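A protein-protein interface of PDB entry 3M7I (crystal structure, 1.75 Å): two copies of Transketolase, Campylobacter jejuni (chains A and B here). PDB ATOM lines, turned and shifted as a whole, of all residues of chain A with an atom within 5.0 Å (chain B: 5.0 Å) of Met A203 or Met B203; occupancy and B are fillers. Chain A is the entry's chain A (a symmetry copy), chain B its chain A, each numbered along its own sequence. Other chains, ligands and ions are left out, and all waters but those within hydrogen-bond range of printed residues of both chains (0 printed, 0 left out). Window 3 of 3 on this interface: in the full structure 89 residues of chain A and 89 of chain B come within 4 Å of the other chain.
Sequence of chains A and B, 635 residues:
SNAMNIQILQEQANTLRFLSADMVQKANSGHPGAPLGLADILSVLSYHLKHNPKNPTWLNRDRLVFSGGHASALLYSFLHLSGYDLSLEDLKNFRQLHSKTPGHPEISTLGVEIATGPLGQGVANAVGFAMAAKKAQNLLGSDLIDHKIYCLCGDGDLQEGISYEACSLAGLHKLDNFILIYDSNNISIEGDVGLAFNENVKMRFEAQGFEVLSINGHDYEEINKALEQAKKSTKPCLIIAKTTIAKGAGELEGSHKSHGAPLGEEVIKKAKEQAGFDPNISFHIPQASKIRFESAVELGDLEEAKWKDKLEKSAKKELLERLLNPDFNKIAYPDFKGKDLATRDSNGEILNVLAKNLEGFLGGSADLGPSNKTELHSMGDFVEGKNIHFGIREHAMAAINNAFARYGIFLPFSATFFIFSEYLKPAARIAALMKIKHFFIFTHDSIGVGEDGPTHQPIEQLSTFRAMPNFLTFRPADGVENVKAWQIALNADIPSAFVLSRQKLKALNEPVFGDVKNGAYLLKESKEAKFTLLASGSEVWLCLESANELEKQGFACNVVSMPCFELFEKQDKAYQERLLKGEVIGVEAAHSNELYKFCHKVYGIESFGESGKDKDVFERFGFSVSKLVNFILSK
N of Ala B207 lies within hydrogen-bond range of SD of Met A203, at 3.6 Å. N of Asn B200 sits at hydrogen-bond distance from O of Ala A207. The backbone NH (N) of Asn A200 is in hydrogen-bond range of the backbone carbonyl oxygen (O) of Ala B207, at 3.0 Å. The backbone NH (N) of Ala A207 is in hydrogen-bond range of the side-chain sulfur (SD) of Met B203 (3.6 Å). SD of Met B203 sits close to O of Met A203 (3.8 Å).
The side-chain amide oxygen (OD1) of Asn B200 sits close to the backbone NH (N) of Lys B202 (3.3 Å). N of Met B203 sits at hydrogen-bond distance from OD1 of Asn B200 (3.0 Å). The backbone NH (N) of Lys A202 sits close to the side-chain amide oxygen (OD1) of Asn A200, 3.3 Å away. OD1 of Asn A200 lies within hydrogen-bond range of N of Met A203, at 3.0 Å.
Arg A204 touches Ala B207 (N to CB, 3.4 Å). Ala A207 touches Arg B204.
Met A203 touches just these residues of chain B: Met B203 and Ala B207. Of chain A, only Met A203 and Ala A207 come within 4 Å of Met B203. Of the printed residues of chain B, Arg A204 touches Ala B207. Printed residues of chain B within 4 Å of Ala A207: Asn B200 (3.0 Å), Met B203 (3.6 Å) and Arg B204 (3.4 Å). Of the printed residues of chain A, Ala B207 touches Asn A200, Met A203 and Arg A204. Of the printed residues of chain A, Asn B200 touches Ala A207.
Of the 8 printed residues of chain B, 4 touch a printed residue of chain A. Hydrophobic or aromatic side chains of chain B within 4 Å of the printed part of chain A: Met B203 and Ala B207. Along chain B the printed residues that touch a printed residue of chain A span positions 200 to 207. Of the 8 printed residues of chain A, 4 touch a printed residue of chain B. Hydrophobic or aromatic side chains of chain A within 4 Å of the printed part of chain B: Met A203 and Ala A207. Among the printed residues, 7 pairs touch across the chains. Among the printed residues, no Asp or Glu carboxylate lies within 4 Å of a Lys or Arg side-chain nitrogen of the other chain.
Asn A200 touches Ala B207, and with the chains exchanged Ala A207 touches Asn B200. Met B203 touches its own counterpart, Met A203. Met A203 touches Ala B207, and with the chains exchanged Ala A207 touches Met B203. Arg A204 touches Ala B207, and with the chains exchanged Ala A207 touches Arg B204.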
ATOM      1  N   ASN A 200      26.456   9.032  -2.844  1.00  0.00           N
ATOM      2  CA  ASN A 200      26.447   9.990  -3.931  1.00  0.00           C
ATOM      3  C   ASN A 200      26.408  11.358  -3.315  1.00  0.00           C
ATOM      4  O   ASN A 200      25.361  11.863  -2.871  1.00  0.00           O
ATOM      5  CB  ASN A 200      25.266   9.758  -4.855  1.00  0.00           C
ATOM      6  CG  ASN A 200      25.267  10.680  -6.024  1.00  0.00           C
ATOM      7  OD1 ASN A 200      25.750  11.803  -5.947  1.00  0.00           O
ATOM      8  ND2 ASN A 200      24.654  10.224  -7.129  1.00  0.00           N
ATOM      9  N   VAL A 201      27.610  11.951  -3.183  1.00  0.00           N
ATOM     10  CA  VAL A 201      27.737  13.165  -2.380  1.00  0.00           C
ATOM     11  C   VAL A 201      27.023  14.321  -3.020  1.00  0.00           C
ATOM     12  O   VAL A 201      26.434  15.140  -2.380  1.00  0.00           O
ATOM     13  CB  VAL A 201      29.240  13.496  -2.132  1.00  0.00           C
ATOM     14  CG1 VAL A 201      29.302  14.895  -1.423  1.00  0.00           C
ATOM     15  CG2 VAL A 201      29.890  12.316  -1.417  1.00  0.00           C
ATOM     16  N   LYS A 202      27.050  14.378  -4.366  1.00  0.00           N
ATOM     17  CA  LYS A 202      26.336  15.406  -5.064  1.00  0.00           C
ATOM     18  C   LYS A 202      24.854  15.338  -4.787  1.00  0.00           C
ATOM     19  O   LYS A 202      24.228  16.370  -4.550  1.00  0.00           O
ATOM     20  CB  LYS A 202      26.606  15.287  -6.580  1.00  0.00           C
ATOM     21  CG  LYS A 202      25.850  16.275  -7.431  1.00  0.00           C
ATOM     22  CD  LYS A 202      26.344  16.125  -8.933  1.00  0.00           C
ATOM     23  CE  LYS A 202      26.056  17.379  -9.774  1.00  0.00           C
ATOM     24  NZ  LYS A 202      24.648  17.556 -10.153  1.00  0.00           N
ATOM     25  N   MET A 203      24.321  14.135  -4.797  1.00  0.00           N
ATOM     26  CA  MET A 203      22.882  13.965  -4.634  1.00  0.00           C
ATOM     27  C   MET A 203      22.506  14.303  -3.159  1.00  0.00           C
ATOM     28  O   MET A 203      21.576  15.003  -2.887  1.00  0.00           O
ATOM     29  CB  MET A 203      22.456  12.549  -5.067  1.00  0.00           C
ATOM     30  CG  MET A 203      20.952  12.439  -5.100  1.00  0.00           C
ATOM     31  SD  MET A 203      20.227  10.721  -5.383  1.00  0.00           S
ATOM     32  CE  MET A 203      21.590   9.832  -6.163  1.00  0.00           C
ATOM     33  N   ARG A 204      23.334  13.868  -2.232  1.00  0.00           N
ATOM     34  CA  ARG A 204      23.198  14.232  -0.836  1.00  0.00           C
ATOM     35  C   ARG A 204      23.043  15.704  -0.620  1.00  0.00           C
ATOM     36  O   ARG A 204      22.151  16.138   0.005  1.00  0.00           O
ATOM     37  CB  ARG A 204      24.403  13.739  -0.043  1.00  0.00           C
ATOM     38  CG  ARG A 204      24.592  14.378   1.324  1.00  0.00           C
ATOM     39  CD  ARG A 204      25.854  13.907   1.947  1.00  0.00           C
ATOM     40  NE  ARG A 204      26.268  14.679   3.095  1.00  0.00           N
ATOM     41  CZ  ARG A 204      27.256  14.340   3.915  1.00  0.00           C
ATOM     42  NH1 ARG A 204      27.894  13.210   3.779  1.00  0.00           N
ATOM     43  NH2 ARG A 204      27.566  15.124   4.900  1.00  0.00           N
ATOM     44  N   PHE A 205      23.964  16.469  -1.133  1.00  0.00           N
ATOM     45  CA  PHE A 205      23.921  17.906  -0.919  1.00  0.00           C
ATOM     46  C   PHE A 205      22.810  18.648  -1.654  1.00  0.00           C
ATOM     47  O   PHE A 205      22.238  19.644  -1.165  1.00  0.00           O
ATOM     48  CB  PHE A 205      25.298  18.515  -1.218  1.00  0.00           C
ATOM     49  CG  PHE A 205      26.244  18.409  -0.014  1.00  0.00           C
ATOM     50  CD1 PHE A 205      26.938  17.232   0.228  1.00  0.00           C
ATOM     51  CD2 PHE A 205      26.378  19.493   0.831  1.00  0.00           C
ATOM     52  CE1 PHE A 205      27.826  17.110   1.315  1.00  0.00           C
ATOM     53  CE2 PHE A 205      27.328  19.388   1.909  1.00  0.00           C
ATOM     54  CZ  PHE A 205      27.972  18.217   2.134  1.00  0.00           C
ATOM     55  N   GLU A 206      22.510  18.167  -2.871  1.00  0.00           N
ATOM     56  CA  GLU A 206      21.393  18.742  -3.583  1.00  0.00           C
ATOM     57  C   GLU A 206      20.080  18.477  -2.832  1.00  0.00           C
ATOM     58  O   GLU A 206      19.191  19.344  -2.764  1.00  0.00           O
ATOM     59  CB  GLU A 206      21.349  18.163  -5.009  1.00  0.00           C
ATOM     60  CG  GLU A 206      22.512  18.718  -5.911  1.00  0.00           C
ATOM     61  CD  GLU A 206      22.612  18.056  -7.323  1.00  0.00           C
ATOM     62  OE1 GLU A 206      23.413  18.549  -8.198  1.00  0.00           O
ATOM     63  OE2 GLU A 206      21.948  17.020  -7.567  1.00  0.00           O
ATOM     64  N   ALA A 207      20.000  17.311  -2.212  1.00  0.00           N
ATOM     65  CA  ALA A 207      18.818  17.006  -1.337  1.00  0.00           C
ATOM     66  C   ALA A 207      18.679  18.013  -0.190  1.00  0.00           C
ATOM     67  O   ALA A 207      17.573  18.277   0.257  1.00  0.00           O
ATOM     68  CB  ALA A 207      18.842  15.575  -0.824  1.00  0.00           C
ATOM     69  N   ASN B 200      14.807  17.206   0.832  1.00  0.00           N
ATOM     70  CA  ASN B 200      14.182  16.221  -0.028  1.00  0.00           C
ATOM     71  C   ASN B 200      14.587  14.869   0.480  1.00  0.00           C
ATOM     72  O   ASN B 200      15.699  14.367   0.236  1.00  0.00           O
ATOM     73  CB  ASN B 200      14.592  16.420  -1.476  1.00  0.00           C
ATOM     74  CG  ASN B 200      13.912  15.470  -2.397  1.00  0.00           C
ATOM     75  OD1 ASN B 200      13.575  14.352  -2.023  1.00  0.00           O
ATOM     76  ND2 ASN B 200      13.754  15.893  -3.663  1.00  0.00           N
ATOM     77  N   VAL B 201      13.697  14.289   1.308  1.00  0.00           N
ATOM     78  CA  VAL B 201      14.077  13.096   2.063  1.00  0.00           C
ATOM     79  C   VAL B 201      14.287  11.919   1.154  1.00  0.00           C
ATOM     80  O   VAL B 201      15.147  11.111   1.346  1.00  0.00           O
ATOM     81  CB  VAL B 201      13.010  12.784   3.155  1.00  0.00           C
ATOM     82  CG1 VAL B 201      13.387  11.403   3.799  1.00  0.00           C
ATOM     83  CG2 VAL B 201      12.895  13.986   4.086  1.00  0.00           C
ATOM     84  N   LYS B 202      13.475  11.829   0.083  1.00  0.00           N
ATOM     85  CA  LYS B 202      13.649  10.778  -0.875  1.00  0.00           C
ATOM     86  C   LYS B 202      15.010  10.841  -1.525  1.00  0.00           C
ATOM     87  O   LYS B 202      15.665   9.809  -1.676  1.00  0.00           O
ATOM     88  CB  LYS B 202      12.538  10.861  -1.945  1.00  0.00           C
ATOM     89  CG  LYS B 202      12.658   9.846  -3.053  1.00  0.00           C
ATOM     90  CD  LYS B 202      11.374   9.963  -3.980  1.00  0.00           C
ATOM     91  CE  LYS B 202      11.123   8.686  -4.799  1.00  0.00           C
ATOM     92  NZ  LYS B 202      12.040   8.489  -5.929  1.00  0.00           N
ATOM     93  N   MET B 203      15.426  12.039  -1.876  1.00  0.00           N
ATOM     94  CA  MET B 203      16.684  12.201  -2.595  1.00  0.00           C
ATOM     95  C   MET B 203      17.858  11.897  -1.614  1.00  0.00           C
ATOM     96  O   MET B 203      18.776  11.196  -1.924  1.00  0.00           O
ATOM     97  CB  MET B 203      16.763  13.603  -3.230  1.00  0.00           C
ATOM     98  CG  MET B 203      17.959  13.699  -4.144  1.00  0.00           C
ATOM     99  SD  MET B 203      18.365  15.404  -4.842  1.00  0.00           S
ATOM    100  CE  MET B 203      16.797  16.284  -4.693  1.00  0.00           C
ATOM    101  N   ARG B 204      17.731  12.361  -0.389  1.00  0.00           N
ATOM    102  CA  ARG B 204      18.664  12.031   0.669  1.00  0.00           C
ATOM    103  C   ARG B 204      18.929  10.563   0.788  1.00  0.00           C
ATOM    104  O   ARG B 204      20.022  10.138   0.780  1.00  0.00           O
ATOM    105  CB  ARG B 204      18.152  12.554   2.006  1.00  0.00           C
ATOM    106  CG  ARG B 204      18.808  11.951   3.238  1.00  0.00           C
ATOM    107  CD  ARG B 204      18.150  12.447   4.472  1.00  0.00           C
ATOM    108  NE  ARG B 204      18.497  11.707   5.663  1.00  0.00           N
ATOM    109  CZ  ARG B 204      18.177  12.075   6.899  1.00  0.00           C
ATOM    110  NH1 ARG B 204      17.571  13.205   7.136  1.00  0.00           N
ATOM    111  NH2 ARG B 204      18.511  11.317   7.896  1.00  0.00           N
ATOM    112  N   PHE B 205      17.888   9.793   0.934  1.00  0.00           N
ATOM    113  CA  PHE B 205      18.060   8.362   1.117  1.00  0.00           C
ATOM    114  C   PHE B 205      18.533   7.593  -0.111  1.00  0.00           C
ATOM    115  O   PHE B 205      19.291   6.605  -0.027  1.00  0.00           O
ATOM    116  CB  PHE B 205      16.776   7.757   1.701  1.00  0.00           C
ATOM    117  CG  PHE B 205      16.717   7.900   3.228  1.00  0.00           C
ATOM    118  CD1 PHE B 205      16.289   9.089   3.802  1.00  0.00           C
ATOM    119  CD2 PHE B 205      17.115   6.839   4.017  1.00  0.00           C
ATOM    120  CE1 PHE B 205      16.209   9.245   5.201  1.00  0.00           C
ATOM    121  CE2 PHE B 205      16.980   6.978   5.444  1.00  0.00           C
ATOM    122  CZ  PHE B 205      16.582   8.160   5.976  1.00  0.00           C
ATOM    123  N   GLU B 206      18.056   8.041  -1.284  1.00  0.00           N
ATOM    124  CA  GLU B 206      18.545   7.440  -2.501  1.00  0.00           C
ATOM    125  C   GLU B 206      20.047   7.713  -2.673  1.00  0.00           C
ATOM    126  O   GLU B 206      20.812   6.840  -3.119  1.00  0.00           O
ATOM    127  CB  GLU B 206      17.737   7.983  -3.695  1.00  0.00           C
ATOM    128  CG  GLU B 206      16.271   7.414  -3.726  1.00  0.00           C
ATOM    129  CD  GLU B 206      15.354   8.043  -4.825  1.00  0.00           C
ATOM    130  OE1 GLU B 206      14.196   7.534  -5.050  1.00  0.00           O
ATOM    131  OE2 GLU B 206      15.740   9.067  -5.439  1.00  0.00           O
ATOM    132  N   ALA B 207      20.467   8.893  -2.248  1.00  0.00           N
ATOM    133  CA  ALA B 207      21.935   9.210  -2.244  1.00  0.00           C
ATOM    134  C   ALA B 207      22.729   8.231  -1.373  1.00  0.00           C
ATOM    135  O   ALA B 207      23.889   7.969  -1.655  1.00  0.00           O
ATOM    136  CB  ALA B 207      22.206  10.653  -1.850  1.00  0.00           C
